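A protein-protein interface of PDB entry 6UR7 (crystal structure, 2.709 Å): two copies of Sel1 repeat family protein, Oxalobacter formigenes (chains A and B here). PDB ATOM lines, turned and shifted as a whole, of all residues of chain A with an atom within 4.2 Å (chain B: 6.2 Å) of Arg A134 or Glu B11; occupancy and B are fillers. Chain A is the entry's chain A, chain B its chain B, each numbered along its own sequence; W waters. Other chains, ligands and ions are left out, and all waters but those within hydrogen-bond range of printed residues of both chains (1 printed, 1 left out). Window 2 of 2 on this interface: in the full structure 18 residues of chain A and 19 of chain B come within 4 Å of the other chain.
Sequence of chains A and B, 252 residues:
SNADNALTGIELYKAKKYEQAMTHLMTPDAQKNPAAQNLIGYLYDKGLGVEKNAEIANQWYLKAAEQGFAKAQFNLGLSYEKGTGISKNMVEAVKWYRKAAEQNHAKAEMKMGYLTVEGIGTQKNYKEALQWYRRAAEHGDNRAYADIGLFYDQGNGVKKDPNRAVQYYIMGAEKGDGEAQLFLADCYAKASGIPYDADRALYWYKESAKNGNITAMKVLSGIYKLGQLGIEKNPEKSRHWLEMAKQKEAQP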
ATOM      1  N   LEU A 130     -14.381 -10.648 -23.871  1.00  0.00           N
ATOM      2  CA  LEU A 130     -14.061 -10.529 -22.453  1.00  0.00           C
ATOM      3  C   LEU A 130     -15.299 -10.731 -21.590  1.00  0.00           C
ATOM      4  O   LEU A 130     -15.206 -11.299 -20.494  1.00  0.00           O
ATOM      5  CB  LEU A 130     -13.423  -9.169 -22.171  1.00  0.00           C
ATOM      6  CG  LEU A 130     -13.017  -8.870 -20.727  1.00  0.00           C
ATOM      7  CD1 LEU A 130     -12.108  -9.958 -20.177  1.00  0.00           C
ATOM      8  CD2 LEU A 130     -12.341  -7.513 -20.636  1.00  0.00           C
ATOM      9  N   GLN A 131     -16.464 -10.294 -22.070  1.00  0.00           N
ATOM     10  CA  GLN A 131     -17.697 -10.504 -21.318  1.00  0.00           C
ATOM     11  C   GLN A 131     -18.047 -11.984 -21.227  1.00  0.00           C
ATOM     12  O   GLN A 131     -18.555 -12.445 -20.198  1.00  0.00           O
ATOM     13  CB  GLN A 131     -18.842  -9.725 -21.960  1.00  0.00           C
ATOM     14  CG  GLN A 131     -18.687  -8.218 -21.878  1.00  0.00           C
ATOM     15  CD  GLN A 131     -19.751  -7.483 -22.668  1.00  0.00           C
ATOM     16  OE1 GLN A 131     -19.966  -7.760 -23.847  1.00  0.00           O
ATOM     17  NE2 GLN A 131     -20.425  -6.541 -22.018  1.00  0.00           N
ATOM     18  N   TRP A 132     -17.779 -12.745 -22.291  1.00  0.00           N
ATOM     19  CA  TRP A 132     -18.092 -14.172 -22.273  1.00  0.00           C
ATOM     20  C   TRP A 132     -17.223 -14.920 -21.268  1.00  0.00           C
ATOM     21  O   TRP A 132     -17.711 -15.805 -20.556  1.00  0.00           O
ATOM     22  CB  TRP A 132     -17.924 -14.771 -23.669  1.00  0.00           C
ATOM     23  CG  TRP A 132     -18.948 -14.305 -24.658  1.00  0.00           C
ATOM     24  CD1 TRP A 132     -18.715 -13.639 -25.825  1.00  0.00           C
ATOM     25  CD2 TRP A 132     -20.369 -14.468 -24.565  1.00  0.00           C
ATOM     26  NE1 TRP A 132     -19.903 -13.383 -26.468  1.00  0.00           N
ATOM     27  CE2 TRP A 132     -20.933 -13.879 -25.713  1.00  0.00           C
ATOM     28  CE3 TRP A 132     -21.220 -15.058 -23.624  1.00  0.00           C
ATOM     29  CZ2 TRP A 132     -22.306 -13.861 -25.945  1.00  0.00           C
ATOM     30  CZ3 TRP A 132     -22.582 -15.038 -23.855  1.00  0.00           C
ATOM     31  CH2 TRP A 132     -23.113 -14.445 -25.008  1.00  0.00           C
ATOM     32  N   TYR A 133     -15.932 -14.585 -21.200  1.00  0.00           N
ATOM     33  CA  TYR A 133     -15.048 -15.276 -20.269  1.00  0.00           C
ATOM     34  C   TYR A 133     -15.391 -14.959 -18.820  1.00  0.00           C
ATOM     35  O   TYR A 133     -15.216 -15.814 -17.945  1.00  0.00           O
ATOM     36  CB  TYR A 133     -13.591 -14.921 -20.558  1.00  0.00           C
ATOM     37  CG  TYR A 133     -12.993 -15.681 -21.721  1.00  0.00           C
ATOM     38  CD1 TYR A 133     -12.701 -15.042 -22.917  1.00  0.00           C
ATOM     39  CD2 TYR A 133     -12.722 -17.039 -21.620  1.00  0.00           C
ATOM     40  CE1 TYR A 133     -12.151 -15.733 -23.980  1.00  0.00           C
ATOM     41  CE2 TYR A 133     -12.173 -17.740 -22.677  1.00  0.00           C
ATOM     42  CZ  TYR A 133     -11.891 -17.082 -23.855  1.00  0.00           C
ATOM     43  OH  TYR A 133     -11.343 -17.774 -24.911  1.00  0.00           O
ATOM     44  N   ARG A 134     -15.871 -13.742 -18.545  1.00  0.00           N
ATOM     45  CA  ARG A 134     -16.295 -13.409 -17.189  1.00  0.00           C
ATOM     46  C   ARG A 134     -17.453 -14.293 -16.750  1.00  0.00           C
ATOM     47  O   ARG A 134     -17.448 -14.841 -15.641  1.00  0.00           O
ATOM     48  CB  ARG A 134     -16.688 -11.935 -17.101  1.00  0.00           C
ATOM     49  CG  ARG A 134     -15.533 -10.957 -17.190  1.00  0.00           C
ATOM     50  CD  ARG A 134     -15.925  -9.629 -16.560  1.00  0.00           C
ATOM     51  NE  ARG A 134     -14.948  -8.576 -16.813  1.00  0.00           N
ATOM     52  CZ  ARG A 134     -15.077  -7.657 -17.765  1.00  0.00           C
ATOM     53  NH1 ARG A 134     -16.143  -7.663 -18.553  1.00  0.00           N
ATOM     54  NH2 ARG A 134     -14.142  -6.731 -17.926  1.00  0.00           N
ATOM     55  N   ARG A 135     -18.462 -14.442 -17.612  1.00  0.00           N
ATOM     56  CA  ARG A 135     -19.590 -15.306 -17.288  1.00  0.00           C
ATOM     57  C   ARG A 135     -19.152 -16.763 -17.185  1.00  0.00           C
ATOM     58  O   ARG A 135     -19.632 -17.501 -16.317  1.00  0.00           O
ATOM     59  CB  ARG A 135     -20.692 -15.140 -18.335  1.00  0.00           C
ATOM     60  CG  ARG A 135     -21.026 -13.684 -18.632  1.00  0.00           C
ATOM     61  CD  ARG A 135     -22.041 -13.533 -19.757  1.00  0.00           C
ATOM     62  NE  ARG A 135     -23.413 -13.733 -19.299  1.00  0.00           N
ATOM     63  CZ  ARG A 135     -24.163 -14.780 -19.624  1.00  0.00           C
ATOM     64  NH1 ARG A 135     -23.681 -15.722 -20.419  1.00  0.00           N
ATOM     65  NH2 ARG A 135     -25.401 -14.880 -19.159  1.00  0.00           N
ATOM     66  N   ALA A 136     -18.229 -17.189 -18.052  1.00  0.00           N
ATOM     67  CA  ALA A 136     -17.746 -18.564 -17.998  1.00  0.00           C
ATOM     68  C   ALA A 136     -17.005 -18.840 -16.695  1.00  0.00           C
ATOM     69  O   ALA A 136     -17.134 -19.925 -16.116  1.00  0.00           O
ATOM     70  CB  ALA A 136     -16.846 -18.854 -19.198  1.00  0.00           C
ATOM     71  N   ALA A 137     -16.220 -17.870 -16.220  1.00  0.00           N
ATOM     72  CA  ALA A 137     -15.539 -18.035 -14.940  1.00  0.00           C
ATOM     73  C   ALA A 137     -16.533 -18.037 -13.788  1.00  0.00           C
ATOM     74  O   ALA A 137     -16.403 -18.829 -12.847  1.00  0.00           O
ATOM     75  CB  ALA A 137     -14.499 -16.932 -14.750  1.00  0.00           C
ATOM     76  N   GLU A 138     -17.534 -17.158 -13.848  1.00  0.00           N
ATOM     77  CA  GLU A 138     -18.538 -17.095 -12.793  1.00  0.00           C
ATOM     78  C   GLU A 138     -19.400 -18.351 -12.759  1.00  0.00           C
ATOM     79  O   GLU A 138     -19.855 -18.760 -11.685  1.00  0.00           O
ATOM     80  CB  GLU A 138     -19.411 -15.855 -12.985  1.00  0.00           C
ATOM     81  CG  GLU A 138     -20.539 -15.717 -11.979  1.00  0.00           C
ATOM     82  CD  GLU A 138     -21.586 -14.716 -12.416  1.00  0.00           C
ATOM     83  OE1 GLU A 138     -21.332 -13.976 -13.391  1.00  0.00           O
ATOM     84  OE2 GLU A 138     -22.666 -14.674 -11.790  1.00  0.00           O
ATOM     85  N   ILE A 148      -9.043 -14.413 -18.904  1.00  0.00           N
ATOM     86  CA  ILE A 148      -9.413 -13.027 -18.631  1.00  0.00           C
ATOM     87  C   ILE A 148      -8.168 -12.172 -18.425  1.00  0.00           C
ATOM     88  O   ILE A 148      -8.077 -11.050 -18.935  1.00  0.00           O
ATOM     89  CB  ILE A 148     -10.354 -12.955 -17.413  1.00  0.00           C
ATOM     90  CG1 ILE A 148     -11.684 -13.645 -17.719  1.00  0.00           C
ATOM     91  CG2 ILE A 148     -10.586 -11.511 -17.000  1.00  0.00           C
ATOM     92  CD1 ILE A 148     -12.627 -13.702 -16.533  1.00  0.00           C
ATOM     93  N   TYR A 152      -5.976  -8.065 -20.020  1.00  0.00           N
ATOM     94  CA  TYR A 152      -5.345  -6.945 -19.332  1.00  0.00           C
ATOM     95  C   TYR A 152      -3.835  -6.938 -19.538  1.00  0.00           C
ATOM     96  O   TYR A 152      -3.226  -5.869 -19.644  1.00  0.00           O
ATOM     97  CB  TYR A 152      -5.679  -6.988 -17.841  1.00  0.00           C
ATOM     98  CG  TYR A 152      -7.149  -6.802 -17.540  1.00  0.00           C
ATOM     99  CD1 TYR A 152      -7.684  -5.532 -17.364  1.00  0.00           C
ATOM    100  CD2 TYR A 152      -7.999  -7.893 -17.433  1.00  0.00           C
ATOM    101  CE1 TYR A 152      -9.027  -5.355 -17.089  1.00  0.00           C
ATOM    102  CE2 TYR A 152      -9.343  -7.726 -17.157  1.00  0.00           C
ATOM    103  CZ  TYR A 152      -9.851  -6.455 -16.986  1.00  0.00           C
ATOM    104  OH  TYR A 152     -11.188  -6.284 -16.712  1.00  0.00           O
ATOM    105  N   ALA B   3     -19.074  -3.542 -26.847  1.00  0.00           N
ATOM    106  CA  ALA B   3     -19.563  -4.587 -25.965  1.00  0.00           C
ATOM    107  C   ALA B   3     -21.044  -4.859 -26.218  1.00  0.00           C
ATOM    108  O   ALA B   3     -21.757  -4.056 -26.824  1.00  0.00           O
ATOM    109  CB  ALA B   3     -19.342  -4.207 -24.500  1.00  0.00           C
ATOM    110  N   ASP B   4     -21.500  -6.016 -25.740  1.00  0.00           N
ATOM    111  CA  ASP B   4     -22.894  -6.409 -25.895  1.00  0.00           C
ATOM    112  C   ASP B   4     -23.755  -5.710 -24.849  1.00  0.00           C
ATOM    113  O   ASP B   4     -23.425  -5.715 -23.659  1.00  0.00           O
ATOM    114  CB  ASP B   4     -23.037  -7.924 -25.769  1.00  0.00           C
ATOM    115  CG  ASP B   4     -24.442  -8.400 -26.068  1.00  0.00           C
ATOM    116  OD1 ASP B   4     -24.784  -8.527 -27.262  1.00  0.00           O
ATOM    117  OD2 ASP B   4     -25.208  -8.644 -25.111  1.00  0.00           O
ATOM    118  N   ALA B   6     -26.829  -6.462 -23.741  1.00  0.00           N
ATOM    119  CA  ALA B   6     -27.429  -7.388 -22.784  1.00  0.00           C
ATOM    120  C   ALA B   6     -26.401  -7.877 -21.773  1.00  0.00           C
ATOM    121  O   ALA B   6     -26.675  -7.917 -20.567  1.00  0.00           O
ATOM    122  CB  ALA B   6     -28.064  -8.566 -23.519  1.00  0.00           C
ATOM    123  N   LEU B   7     -25.208  -8.246 -22.243  1.00  0.00           N
ATOM    124  CA  LEU B   7     -24.165  -8.707 -21.333  1.00  0.00           C
ATOM    125  C   LEU B   7     -23.701  -7.586 -20.411  1.00  0.00           C
ATOM    126  O   LEU B   7     -23.396  -7.827 -19.238  1.00  0.00           O
ATOM    127  CB  LEU B   7     -22.990  -9.275 -22.128  1.00  0.00           C
ATOM    128  CG  LEU B   7     -22.996 -10.774 -22.454  1.00  0.00           C
ATOM    129  CD1 LEU B   7     -24.357 -11.248 -22.935  1.00  0.00           C
ATOM    130  CD2 LEU B   7     -21.930 -11.082 -23.492  1.00  0.00           C
ATOM    131  N   THR B   8     -23.646  -6.353 -20.922  1.00  0.00           N
ATOM    132  CA  THR B   8     -23.271  -5.221 -20.081  1.00  0.00           C
ATOM    133  C   THR B   8     -24.319  -4.961 -19.006  1.00  0.00           C
ATOM    134  O   THR B   8     -23.976  -4.679 -17.853  1.00  0.00           O
ATOM    135  CB  THR B   8     -23.067  -3.969 -20.939  1.00  0.00           C
ATOM    136  OG1 THR B   8     -22.056  -4.221 -21.924  1.00  0.00           O
ATOM    137  CG2 THR B   8     -22.641  -2.790 -20.076  1.00  0.00           C
ATOM    138  N   GLY B   9     -25.601  -5.057 -19.362  1.00  0.00           N
ATOM    139  CA  GLY B   9     -26.648  -4.829 -18.382  1.00  0.00           C
ATOM    140  C   GLY B   9     -26.667  -5.867 -17.277  1.00  0.00           C
ATOM    141  O   GLY B   9     -26.988  -5.550 -16.129  1.00  0.00           O
ATOM    142  N   ILE B  10     -26.317  -7.114 -17.601  1.00  0.00           N
ATOM    143  CA  ILE B  10     -26.338  -8.176 -16.600  1.00  0.00           C
ATOM    144  C   ILE B  10     -25.237  -7.958 -15.567  1.00  0.00           C
ATOM    145  O   ILE B  10     -25.468  -8.073 -14.357  1.00  0.00           O
ATOM    146  CB  ILE B  10     -26.218  -9.553 -17.277  1.00  0.00           C
ATOM    147  CG1 ILE B  10     -27.458  -9.830 -18.131  1.00  0.00           C
ATOM    148  CG2 ILE B  10     -26.033 -10.647 -16.236  1.00  0.00           C
ATOM    149  CD1 ILE B  10     -27.410 -11.146 -18.867  1.00  0.00           C
ATOM    150  N   GLU B  11     -24.026  -7.636 -16.023  1.00  0.00           N
ATOM    151  CA  GLU B  11     -22.951  -7.347 -15.082  1.00  0.00           C
ATOM    152  C   GLU B  11     -23.172  -6.029 -14.350  1.00  0.00           C
ATOM    153  O   GLU B  11     -22.665  -5.859 -13.237  1.00  0.00           O
ATOM    154  CB  GLU B  11     -21.600  -7.350 -15.800  1.00  0.00           C
ATOM    155  CG  GLU B  11     -21.506  -6.409 -16.988  1.00  0.00           C
ATOM    156  CD  GLU B  11     -20.326  -6.727 -17.887  1.00  0.00           C
ATOM    157  OE1 GLU B  11     -19.752  -7.828 -17.746  1.00  0.00           O
ATOM    158  OE2 GLU B  11     -19.972  -5.879 -18.733  1.00  0.00           O
ATOM    159  N   LEU B  12     -23.931  -5.102 -14.939  1.00  0.00           N
ATOM    160  CA  LEU B  12     -24.303  -3.894 -14.211  1.00  0.00           C
ATOM    161  C   LEU B  12     -25.267  -4.214 -13.077  1.00  0.00           C
ATOM    162  O   LEU B  12     -25.161  -3.643 -11.986  1.00  0.00           O
ATOM    163  CB  LEU B  12     -24.918  -2.868 -15.161  1.00  0.00           C
ATOM    164  CG  LEU B  12     -23.952  -2.032 -16.004  1.00  0.00           C
ATOM    165  CD1 LEU B  12     -24.719  -1.158 -16.986  1.00  0.00           C
ATOM    166  CD2 LEU B  12     -23.059  -1.183 -15.113  1.00  0.00           C
ATOM    167  N   TYR B  13     -26.220  -5.119 -13.318  1.00  0.00           N
ATOM    168  CA  TYR B  13     -27.098  -5.570 -12.244  1.00  0.00           C
ATOM    169  C   TYR B  13     -26.307  -6.271 -11.148  1.00  0.00           C
ATOM    170  O   TYR B  13     -26.566  -6.070  -9.956  1.00  0.00           O
ATOM    171  CB  TYR B  13     -28.180  -6.498 -12.799  1.00  0.00           C
ATOM    172  CG  TYR B  13     -28.775  -7.424 -11.760  1.00  0.00           C
ATOM    173  CD1 TYR B  13     -29.744  -6.976 -10.874  1.00  0.00           C
ATOM    174  CD2 TYR B  13     -28.365  -8.749 -11.664  1.00  0.00           C
ATOM    175  CE1 TYR B  13     -30.288  -7.817  -9.920  1.00  0.00           C
ATOM    176  CE2 TYR B  13     -28.903  -9.598 -10.715  1.00  0.00           C
ATOM    177  CZ  TYR B  13     -29.864  -9.128  -9.845  1.00  0.00           C
ATOM    178  OH  TYR B  13     -30.403  -9.969  -8.899  1.00  0.00           O
ATOM    179  N   LYS B  14     -25.337  -7.105 -11.534  1.00  0.00           N
ATOM    180  CA  LYS B  14     -24.522  -7.801 -10.545  1.00  0.00           C
ATOM    181  C   LYS B  14     -23.676  -6.831  -9.733  1.00  0.00           C
ATOM    182  O   LYS B  14     -23.331  -7.121  -8.581  1.00  0.00           O
ATOM    183  CB  LYS B  14     -23.634  -8.836 -11.233  1.00  0.00           C
ATOM    184  CG  LYS B  14     -24.403  -9.964 -11.902  1.00  0.00           C
ATOM    185  CD  LYS B  14     -23.463 -10.933 -12.594  1.00  0.00           C
ATOM    186  CE  LYS B  14     -22.372 -11.403 -11.646  1.00  0.00           C
ATOM    187  NZ  LYS B  14     -22.936 -12.036 -10.422  1.00  0.00           N
ATOM    188  N   ALA B  15     -23.334  -5.681 -10.309  1.00  0.00           N
ATOM    189  CA  ALA B  15     -22.646  -4.622  -9.582  1.00  0.00           C
ATOM    190  C   ALA B  15     -23.591  -3.787  -8.729  1.00  0.00           C
ATOM    191  O   ALA B  15     -23.155  -2.791  -8.141  1.00  0.00           O
ATOM    192  CB  ALA B  15     -21.892  -3.715 -10.560  1.00  0.00           C
ATOM    193  N   LYS B  16     -24.868  -4.173  -8.662  1.00  0.00           N
ATOM    194  CA  LYS B  16     -25.879  -3.466  -7.874  1.00  0.00           C
ATOM    195  C   LYS B  16     -26.046  -2.024  -8.351  1.00  0.00           C
ATOM    196  O   LYS B  16     -26.277  -1.108  -7.561  1.00  0.00           O
ATOM    197  CB  LYS B  16     -25.554  -3.529  -6.379  1.00  0.00           C
ATOM    198  CG  LYS B  16     -25.414  -4.955  -5.860  1.00  0.00           C
ATOM    199  CD  LYS B  16     -24.992  -5.001  -4.400  1.00  0.00           C
ATOM    200  CE  LYS B  16     -24.789  -6.439  -3.941  1.00  0.00           C
ATOM    201  NZ  LYS B  16     -24.354  -6.526  -2.519  1.00  0.00           N
ATOM    202  N   LEU B  39     -34.149 -10.675 -16.532  1.00  0.00           N
ATOM    203  CA  LEU B  39     -33.649  -9.638 -15.637  1.00  0.00           C
ATOM    204  C   LEU B  39     -34.514  -8.385 -15.696  1.00  0.00           C
ATOM    205  O   LEU B  39     -34.694  -7.710 -14.676  1.00  0.00           O
ATOM    206  CB  LEU B  39     -32.196  -9.310 -15.983  1.00  0.00           C
ATOM    207  CG  LEU B  39     -31.445  -8.368 -15.039  1.00  0.00           C
ATOM    208  CD1 LEU B  39     -31.528  -8.867 -13.606  1.00  0.00           C
ATOM    209  CD2 LEU B  39     -29.997  -8.231 -15.476  1.00  0.00           C
HETATM  210  O   HOH W   1     -22.915 -10.631 -18.472  1.00  0.00           O
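The guanidinium group (NH1) of Arg A134 is in salt-bridge range of the side-chain carboxylate (OE1) of Glu B11.
N of Asp B4 lies within hydrogen-bond range of OE1 of Gln A131, at 3.0 Å.
The side-chain amino group (NZ) of Lys B14 is in salt-bridge range of the side-chain carboxylate (OE2) of Glu A138.
The side-chain amide nitrogen of Gln A131 lies within hydrogen-bond range of the side-chain hydroxyl of Thr B8 (2.8 Å).
The side-chain carboxylate (OE2) of Glu B11 is in hydrogen-bond range of the side-chain amide nitrogen (NE2) of Gln A131 (3.4 Å).
NH2 of Arg A134 lies within hydrogen-bond range of OH of Tyr A152 (3.2 Å).
The backbone carbonyl oxygen (O) of Asp B4 sits at hydrogen-bond distance from the side-chain hydroxyl (OG1) of Thr B8, 2.7 Å away.
The backbone NH (N) of Leu B7 is in hydrogen-bond range of the side-chain carboxylate (OD2) of Asp B4, at 2.9 Å.
The backbone NH of Ala B6 sits at hydrogen-bond distance from the side-chain carboxylate of Asp B4 (3.0 Å).
Among the printed residues, pairs that only touch across the chains: Gln A131 with Ala B3 (3.6 Å), Gln A131 with Leu B7 (3.7 Å), Trp A132 with Leu B7 (3.7 Å) and Arg A135 with Leu B7 (3.97 Å).
Of the printed residues of chain B, Trp A132 touches Leu B7 (3.7 Å).
Arg A134 touches just one residue of chain B: Glu B11 (3.7 Å).
Printed residues of chain B within 4 Å of Glu A138: Lys B14.
Glu B11 touches just these residues of chain A: Gln A131 (3.4 Å) and Arg A134 (3.7 Å).
Tyr B13 touches none of the printed residues of chain A.
The nearest printed residue of chain A that does not touch Glu B11 is Arg A135 (6.1 Å).
The nearest printed residue of chain B that does not touch Trp A132 is Asp B4 (5.9 Å).
Of the 11 printed residues of chain A, 5 touch a printed residue of chain B.
Hydrophobic or aromatic side chains of chain B within 4 Å of the printed part of chain A: Ala B3 and Leu B7.
Among the printed residues, Asp or Glu carboxylates within 4 Å of a Lys or Arg side-chain nitrogen of the other chain: Arg A134 with Glu B11 (3.7 Å) and Glu A138 with Lys B14 (3.0 Å).
No position is printed for both chains.
Of the 9 pairs that touch across the chains among the printed residues, none has its exchanged pair printed and touching as well.
Water W1 lies within hydrogen-bond range of the backbone carbonyl oxygen of Leu B7 (2.9 Å) and the guanidinium group of Arg A135 (3.2 Å).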
